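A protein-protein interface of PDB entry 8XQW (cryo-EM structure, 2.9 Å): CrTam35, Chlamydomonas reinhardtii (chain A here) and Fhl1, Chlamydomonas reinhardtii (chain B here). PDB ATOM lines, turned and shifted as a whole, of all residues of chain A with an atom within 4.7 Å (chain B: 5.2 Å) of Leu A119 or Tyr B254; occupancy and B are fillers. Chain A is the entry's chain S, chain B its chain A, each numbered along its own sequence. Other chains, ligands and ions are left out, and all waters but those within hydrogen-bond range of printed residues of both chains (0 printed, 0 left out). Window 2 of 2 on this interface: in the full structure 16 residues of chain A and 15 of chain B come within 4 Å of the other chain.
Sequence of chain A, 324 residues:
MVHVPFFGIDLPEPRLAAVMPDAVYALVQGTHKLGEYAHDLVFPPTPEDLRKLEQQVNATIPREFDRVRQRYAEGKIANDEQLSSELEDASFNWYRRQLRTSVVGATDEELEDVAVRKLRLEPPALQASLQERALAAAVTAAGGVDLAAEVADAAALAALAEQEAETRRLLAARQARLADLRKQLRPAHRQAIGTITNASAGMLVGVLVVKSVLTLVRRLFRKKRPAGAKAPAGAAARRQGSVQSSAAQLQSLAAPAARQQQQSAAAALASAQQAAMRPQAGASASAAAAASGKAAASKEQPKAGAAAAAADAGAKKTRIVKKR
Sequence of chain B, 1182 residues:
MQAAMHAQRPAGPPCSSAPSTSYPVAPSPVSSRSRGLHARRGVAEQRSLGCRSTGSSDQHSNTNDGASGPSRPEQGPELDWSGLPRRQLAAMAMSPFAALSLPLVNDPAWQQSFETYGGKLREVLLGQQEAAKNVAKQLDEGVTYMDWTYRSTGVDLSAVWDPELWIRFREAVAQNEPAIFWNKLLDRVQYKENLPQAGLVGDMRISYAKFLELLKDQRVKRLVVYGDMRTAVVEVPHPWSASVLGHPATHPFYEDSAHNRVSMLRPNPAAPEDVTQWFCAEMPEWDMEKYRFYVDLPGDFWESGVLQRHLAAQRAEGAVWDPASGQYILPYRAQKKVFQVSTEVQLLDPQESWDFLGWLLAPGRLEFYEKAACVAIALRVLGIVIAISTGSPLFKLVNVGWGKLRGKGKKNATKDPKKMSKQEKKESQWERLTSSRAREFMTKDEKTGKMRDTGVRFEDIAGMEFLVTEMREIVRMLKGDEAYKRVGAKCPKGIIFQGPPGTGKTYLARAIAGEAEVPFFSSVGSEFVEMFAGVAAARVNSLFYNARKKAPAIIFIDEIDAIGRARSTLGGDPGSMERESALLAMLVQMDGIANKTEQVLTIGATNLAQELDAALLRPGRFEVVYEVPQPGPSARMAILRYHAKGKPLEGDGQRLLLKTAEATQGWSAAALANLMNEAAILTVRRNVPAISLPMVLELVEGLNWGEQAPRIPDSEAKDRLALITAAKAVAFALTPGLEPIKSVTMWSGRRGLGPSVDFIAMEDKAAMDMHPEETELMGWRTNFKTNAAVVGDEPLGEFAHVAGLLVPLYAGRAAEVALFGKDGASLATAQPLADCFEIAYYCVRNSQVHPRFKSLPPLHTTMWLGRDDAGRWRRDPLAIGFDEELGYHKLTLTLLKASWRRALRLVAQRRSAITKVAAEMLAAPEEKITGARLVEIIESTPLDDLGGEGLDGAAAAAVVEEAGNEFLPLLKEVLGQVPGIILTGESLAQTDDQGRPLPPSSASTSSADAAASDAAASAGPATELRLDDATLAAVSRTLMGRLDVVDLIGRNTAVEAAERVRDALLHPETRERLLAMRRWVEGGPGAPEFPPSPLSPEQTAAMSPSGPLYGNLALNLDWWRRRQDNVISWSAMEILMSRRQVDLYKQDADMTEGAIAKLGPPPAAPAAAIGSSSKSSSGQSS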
ATOM      1  N   ALA A 115     -30.986 -27.940  16.051  1.00  0.00           N
ATOM      2  CA  ALA A 115     -29.538 -27.754  16.090  1.00  0.00           C
ATOM      3  C   ALA A 115     -28.980 -28.066  17.469  1.00  0.00           C
ATOM      4  O   ALA A 115     -27.949 -28.731  17.591  1.00  0.00           O
ATOM      5  CB  ALA A 115     -29.172 -26.332  15.678  1.00  0.00           C
ATOM      6  N   VAL A 116     -29.649 -27.600  18.523  1.00  0.00           N
ATOM      7  CA  VAL A 116     -29.168 -27.890  19.870  1.00  0.00           C
ATOM      8  C   VAL A 116     -29.457 -29.337  20.249  1.00  0.00           C
ATOM      9  O   VAL A 116     -28.876 -29.867  21.200  1.00  0.00           O
ATOM     10  CB  VAL A 116     -29.775 -26.912  20.890  1.00  0.00           C
ATOM     11  CG1 VAL A 116     -29.626 -25.491  20.408  1.00  0.00           C
ATOM     12  CG2 VAL A 116     -31.225 -27.246  21.150  1.00  0.00           C
ATOM     13  N   ARG A 117     -30.361 -29.998  19.529  1.00  0.00           N
ATOM     14  CA  ARG A 117     -30.581 -31.414  19.788  1.00  0.00           C
ATOM     15  C   ARG A 117     -29.468 -32.262  19.194  1.00  0.00           C
ATOM     16  O   ARG A 117     -28.964 -33.177  19.852  1.00  0.00           O
ATOM     17  CB  ARG A 117     -31.936 -31.849  19.234  1.00  0.00           C
ATOM     18  CG  ARG A 117     -32.291 -33.291  19.534  1.00  0.00           C
ATOM     19  CD  ARG A 117     -32.487 -34.089  18.261  1.00  0.00           C
ATOM     20  NE  ARG A 117     -33.469 -33.471  17.376  1.00  0.00           N
ATOM     21  CZ  ARG A 117     -33.731 -33.887  16.140  1.00  0.00           C
ATOM     22  NH1 ARG A 117     -33.089 -34.932  15.638  1.00  0.00           N
ATOM     23  NH2 ARG A 117     -34.641 -33.262  15.406  1.00  0.00           N
ATOM     24  N   LYS A 118     -29.071 -31.986  17.958  1.00  0.00           N
ATOM     25  CA  LYS A 118     -28.068 -32.812  17.301  1.00  0.00           C
ATOM     26  C   LYS A 118     -26.645 -32.314  17.515  1.00  0.00           C
ATOM     27  O   LYS A 118     -25.710 -32.918  16.986  1.00  0.00           O
ATOM     28  CB  LYS A 118     -28.363 -32.921  15.804  1.00  0.00           C
ATOM     29  CG  LYS A 118     -28.369 -31.611  15.064  1.00  0.00           C
ATOM     30  CD  LYS A 118     -28.295 -31.837  13.567  1.00  0.00           C
ATOM     31  CE  LYS A 118     -29.318 -32.850  13.103  1.00  0.00           C
ATOM     32  NZ  LYS A 118     -29.122 -33.190  11.672  1.00  0.00           N
ATOM     33  N   LEU A 119     -26.457 -31.234  18.266  1.00  0.00           N
ATOM     34  CA  LEU A 119     -25.138 -30.819  18.715  1.00  0.00           C
ATOM     35  C   LEU A 119     -24.884 -31.186  20.165  1.00  0.00           C
ATOM     36  O   LEU A 119     -23.788 -30.934  20.671  1.00  0.00           O
ATOM     37  CB  LEU A 119     -24.960 -29.310  18.538  1.00  0.00           C
ATOM     38  CG  LEU A 119     -24.295 -28.832  17.256  1.00  0.00           C
ATOM     39  CD1 LEU A 119     -24.110 -27.335  17.288  1.00  0.00           C
ATOM     40  CD2 LEU A 119     -22.971 -29.527  17.091  1.00  0.00           C
ATOM     41  N   ARG A 120     -25.879 -31.758  20.844  1.00  0.00           N
ATOM     42  CA  ARG A 120     -25.763 -32.167  22.242  1.00  0.00           C
ATOM     43  C   ARG A 120     -25.226 -31.032  23.109  1.00  0.00           C
ATOM     44  O   ARG A 120     -24.302 -31.212  23.904  1.00  0.00           O
ATOM     45  CB  ARG A 120     -24.900 -33.419  22.376  1.00  0.00           C
ATOM     46  CG  ARG A 120     -25.536 -34.665  21.794  1.00  0.00           C
ATOM     47  CD  ARG A 120     -24.591 -35.849  21.854  1.00  0.00           C
ATOM     48  NE  ARG A 120     -24.308 -36.252  23.226  1.00  0.00           N
ATOM     49  CZ  ARG A 120     -23.160 -36.014  23.850  1.00  0.00           C
ATOM     50  NH1 ARG A 120     -22.186 -35.372  23.223  1.00  0.00           N
ATOM     51  NH2 ARG A 120     -22.987 -36.414  25.101  1.00  0.00           N
ATOM     52  N   LEU A 121     -25.813 -29.851  22.951  1.00  0.00           N
ATOM     53  CA  LEU A 121     -25.410 -28.704  23.748  1.00  0.00           C
ATOM     54  C   LEU A 121     -26.083 -28.656  25.109  1.00  0.00           C
ATOM     55  O   LEU A 121     -25.570 -27.989  26.012  1.00  0.00           O
ATOM     56  CB  LEU A 121     -25.717 -27.404  23.009  1.00  0.00           C
ATOM     57  CG  LEU A 121     -24.900 -27.139  21.755  1.00  0.00           C
ATOM     58  CD1 LEU A 121     -24.958 -25.664  21.416  1.00  0.00           C
ATOM     59  CD2 LEU A 121     -23.474 -27.593  21.960  1.00  0.00           C
ATOM     60  N   VAL B 244     -16.764 -25.751  14.884  1.00  0.00           N
ATOM     61  CA  VAL B 244     -18.159 -25.537  14.528  1.00  0.00           C
ATOM     62  C   VAL B 244     -18.254 -24.123  13.966  1.00  0.00           C
ATOM     63  O   VAL B 244     -19.261 -23.429  14.126  1.00  0.00           O
ATOM     64  CB  VAL B 244     -19.088 -25.772  15.732  1.00  0.00           C
ATOM     65  CG1 VAL B 244     -20.551 -25.665  15.349  1.00  0.00           C
ATOM     66  CG2 VAL B 244     -18.830 -27.130  16.311  1.00  0.00           C
ATOM     67  N   PRO B 252     -24.236 -28.296   5.350  1.00  0.00           N
ATOM     68  CA  PRO B 252     -25.017 -27.551   6.357  1.00  0.00           C
ATOM     69  C   PRO B 252     -25.725 -28.470   7.347  1.00  0.00           C
ATOM     70  O   PRO B 252     -26.912 -28.761   7.256  1.00  0.00           O
ATOM     71  CB  PRO B 252     -26.010 -26.767   5.497  1.00  0.00           C
ATOM     72  CG  PRO B 252     -25.426 -26.765   4.129  1.00  0.00           C
ATOM     73  CD  PRO B 252     -24.754 -28.078   3.995  1.00  0.00           C
ATOM     74  N   PHE B 253     -24.963 -28.943   8.333  1.00  0.00           N
ATOM     75  CA  PHE B 253     -25.518 -29.873   9.310  1.00  0.00           C
ATOM     76  C   PHE B 253     -26.474 -29.167  10.262  1.00  0.00           C
ATOM     77  O   PHE B 253     -27.577 -29.657  10.528  1.00  0.00           O
ATOM     78  CB  PHE B 253     -24.395 -30.539  10.099  1.00  0.00           C
ATOM     79  CG  PHE B 253     -23.738 -31.685   9.394  1.00  0.00           C
ATOM     80  CD1 PHE B 253     -24.305 -32.941   9.413  1.00  0.00           C
ATOM     81  CD2 PHE B 253     -22.536 -31.515   8.744  1.00  0.00           C
ATOM     82  CE1 PHE B 253     -23.698 -33.996   8.779  1.00  0.00           C
ATOM     83  CE2 PHE B 253     -21.926 -32.568   8.113  1.00  0.00           C
ATOM     84  CZ  PHE B 253     -22.509 -33.807   8.126  1.00  0.00           C
ATOM     85  N   TYR B 254     -26.064 -28.019  10.793  1.00  0.00           N
ATOM     86  CA  TYR B 254     -26.771 -27.342  11.872  1.00  0.00           C
ATOM     87  C   TYR B 254     -27.131 -25.933  11.438  1.00  0.00           C
ATOM     88  O   TYR B 254     -26.244 -25.127  11.143  1.00  0.00           O
ATOM     89  CB  TYR B 254     -25.915 -27.305  13.135  1.00  0.00           C
ATOM     90  CG  TYR B 254     -25.045 -28.526  13.296  1.00  0.00           C
ATOM     91  CD1 TYR B 254     -25.570 -29.712  13.774  1.00  0.00           C
ATOM     92  CD2 TYR B 254     -23.705 -28.496  12.953  1.00  0.00           C
ATOM     93  CE1 TYR B 254     -24.789 -30.826  13.910  1.00  0.00           C
ATOM     94  CE2 TYR B 254     -22.916 -29.609  13.092  1.00  0.00           C
ATOM     95  CZ  TYR B 254     -23.464 -30.771  13.569  1.00  0.00           C
ATOM     96  OH  TYR B 254     -22.684 -31.890  13.709  1.00  0.00           O
ATOM     97  N   GLU B 255     -28.428 -25.631  11.422  1.00  0.00           N
ATOM     98  CA  GLU B 255     -28.930 -24.393  10.852  1.00  0.00           C
ATOM     99  C   GLU B 255     -29.818 -23.657  11.842  1.00  0.00           C
ATOM    100  O   GLU B 255     -30.484 -24.257  12.687  1.00  0.00           O
ATOM    101  CB  GLU B 255     -29.717 -24.654   9.565  1.00  0.00           C
ATOM    102  CG  GLU B 255     -28.858 -24.940   8.353  1.00  0.00           C
ATOM    103  CD  GLU B 255     -29.506 -25.933   7.413  1.00  0.00           C
ATOM    104  OE1 GLU B 255     -30.035 -26.952   7.900  1.00  0.00           O
ATOM    105  OE2 GLU B 255     -29.494 -25.693   6.188  1.00  0.00           O
ATOM    106  N   ASP B 256     -29.826 -22.337  11.699  1.00  0.00           N
ATOM    107  CA  ASP B 256     -30.712 -21.437  12.417  1.00  0.00           C
ATOM    108  C   ASP B 256     -32.112 -21.548  11.815  1.00  0.00           C
ATOM    109  O   ASP B 256     -32.328 -22.284  10.850  1.00  0.00           O
ATOM    110  CB  ASP B 256     -30.134 -20.024  12.346  1.00  0.00           C
ATOM    111  CG  ASP B 256     -30.987 -18.994  13.050  1.00  0.00           C
ATOM    112  OD1 ASP B 256     -31.824 -19.386  13.883  1.00  0.00           O
ATOM    113  OD2 ASP B 256     -30.829 -17.790  12.758  1.00  0.00           O
ATOM    114  N   ASN B 260     -29.199 -20.250   8.334  1.00  0.00           N
ATOM    115  CA  ASN B 260     -27.781 -19.924   8.388  1.00  0.00           C
ATOM    116  C   ASN B 260     -27.052 -20.916   9.284  1.00  0.00           C
ATOM    117  O   ASN B 260     -27.558 -21.296  10.343  1.00  0.00           O
ATOM    118  CB  ASN B 260     -27.556 -18.508   8.917  1.00  0.00           C
ATOM    119  CG  ASN B 260     -27.897 -17.454   7.902  1.00  0.00           C
ATOM    120  OD1 ASN B 260     -28.240 -17.767   6.766  1.00  0.00           O
ATOM    121  ND2 ASN B 260     -27.799 -16.193   8.301  1.00  0.00           N
ATOM    122  N   ARG B 261     -25.866 -21.331   8.853  1.00  0.00           N
ATOM    123  CA  ARG B 261     -25.042 -22.199   9.678  1.00  0.00           C
ATOM    124  C   ARG B 261     -24.729 -21.514  11.000  1.00  0.00           C
ATOM    125  O   ARG B 261     -24.502 -20.303  11.051  1.00  0.00           O
ATOM    126  CB  ARG B 261     -23.742 -22.540   8.958  1.00  0.00           C
ATOM    127  CG  ARG B 261     -23.906 -23.213   7.618  1.00  0.00           C
ATOM    128  CD  ARG B 261     -22.597 -23.152   6.867  1.00  0.00           C
ATOM    129  NE  ARG B 261     -22.461 -24.220   5.892  1.00  0.00           N
ATOM    130  CZ  ARG B 261     -22.620 -24.053   4.587  1.00  0.00           C
ATOM    131  NH1 ARG B 261     -22.926 -22.861   4.108  1.00  0.00           N
ATOM    132  NH2 ARG B 261     -22.474 -25.078   3.764  1.00  0.00           N
ATOM    133  N   VAL B 262     -24.715 -22.291  12.075  1.00  0.00           N
ATOM    134  CA  VAL B 262     -24.410 -21.727  13.379  1.00  0.00           C
ATOM    135  C   VAL B 262     -22.902 -21.682  13.585  1.00  0.00           C
ATOM    136  O   VAL B 262     -22.139 -22.434  12.980  1.00  0.00           O
ATOM    137  CB  VAL B 262     -25.095 -22.517  14.501  1.00  0.00           C
ATOM    138  CG1 VAL B 262     -26.509 -22.028  14.685  1.00  0.00           C
ATOM    139  CG2 VAL B 262     -25.086 -23.981  14.173  1.00  0.00           C
ATOM    140  N   MET B 264     -19.824 -20.879  16.901  1.00  0.00           N
ATOM    141  CA  MET B 264     -19.647 -20.954  18.345  1.00  0.00           C
ATOM    142  C   MET B 264     -18.377 -20.253  18.807  1.00  0.00           C
ATOM    143  O   MET B 264     -17.907 -20.515  19.914  1.00  0.00           O
ATOM    144  CB  MET B 264     -19.629 -22.406  18.820  1.00  0.00           C
ATOM    145  CG  MET B 264     -20.770 -23.256  18.304  1.00  0.00           C
ATOM    146  SD  MET B 264     -22.219 -23.209  19.364  1.00  0.00           S
ATOM    147  CE  MET B 264     -21.600 -24.053  20.812  1.00  0.00           C
ATOM    148  N   MET B 283     -16.944 -30.191  16.581  1.00  0.00           N
ATOM    149  CA  MET B 283     -18.028 -30.915  15.954  1.00  0.00           C
ATOM    150  C   MET B 283     -18.097 -32.337  16.501  1.00  0.00           C
ATOM    151  O   MET B 283     -17.075 -32.910  16.873  1.00  0.00           O
ATOM    152  CB  MET B 283     -17.821 -30.947  14.446  1.00  0.00           C
ATOM    153  CG  MET B 283     -19.074 -31.158  13.646  1.00  0.00           C
ATOM    154  SD  MET B 283     -18.783 -31.237  11.874  1.00  0.00           S
ATOM    155  CE  MET B 283     -18.444 -29.523  11.515  1.00  0.00           C
ATOM    156  N   PRO B 284     -19.292 -32.917  16.595  1.00  0.00           N
ATOM    157  CA  PRO B 284     -19.389 -34.326  16.981  1.00  0.00           C
ATOM    158  C   PRO B 284     -18.673 -35.207  15.976  1.00  0.00           C
ATOM    159  O   PRO B 284     -18.694 -34.943  14.775  1.00  0.00           O
ATOM    160  CB  PRO B 284     -20.894 -34.584  16.984  1.00  0.00           C
ATOM    161  CG  PRO B 284     -21.483 -33.271  17.239  1.00  0.00           C
ATOM    162  CD  PRO B 284     -20.612 -32.279  16.551  1.00  0.00           C
ATOM    163  N   ASP B 287     -19.941 -36.426  12.460  1.00  0.00           N
ATOM    164  CA  ASP B 287     -20.216 -35.459  11.410  1.00  0.00           C
ATOM    165  C   ASP B 287     -18.957 -34.913  10.760  1.00  0.00           C
ATOM    166  O   ASP B 287     -19.009 -33.853  10.139  1.00  0.00           O
ATOM    167  CB  ASP B 287     -21.027 -34.301  11.976  1.00  0.00           C
ATOM    168  CG  ASP B 287     -22.450 -34.682  12.268  1.00  0.00           C
ATOM    169  OD1 ASP B 287     -22.837 -35.816  11.934  1.00  0.00           O
ATOM    170  OD2 ASP B 287     -23.186 -33.851  12.833  1.00  0.00           O
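The backbone carbonyl oxygen (O) of Tyr B254 is in hydrogen-bond range of the backbone NH (N) of Val B262, 3.4 Å away.
CB of Ala A115 touches O of Glu B255 (3.9 Å).
CD of Lys A118 touches O of Phe B253, at 3.8 Å.
Lys A118 touches Tyr B254 (CD to CD1, 3.5 Å).
Leu A119 touches Tyr B254.
Leu A119 touches Pro B284 (CD2 to CD, 3.7 Å).
Leu A121 touches Met B264.
Of the printed residues of chain B, Ala A115 touches Glu B255.
Of chain B, only Tyr B254 (3.8 Å) and Pro B284 (3.7 Å) come within 4 Å of Leu A119.
Printed residues of chain A within 4 Å of Phe B253: Lys A118 (3.8 Å).
Printed residues of chain A within 4 Å of Tyr B254: Lys A118 (3.5 Å) and Leu A119 (3.8 Å).
Printed residues of chain A within 4 Å of Met B264: Leu A121 (3.8 Å).
Printed residues of chain A within 4 Å of Pro B284: Leu A119.
The nearest printed residue of chain B that does not touch Leu A121 is Val B244 (7.3 Å).
Of the 13 printed residues of chain B, 5 touch a printed residue of chain A.
Hydrophobic or aromatic side chains of chain B within 4 Å of the printed part of chain A: Tyr B254, Met B264 and Pro B284.
Of the 7 printed residues of chain A, 4 touch a printed residue of chain B.
Among the printed residues, 6 pairs touch across the chains.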
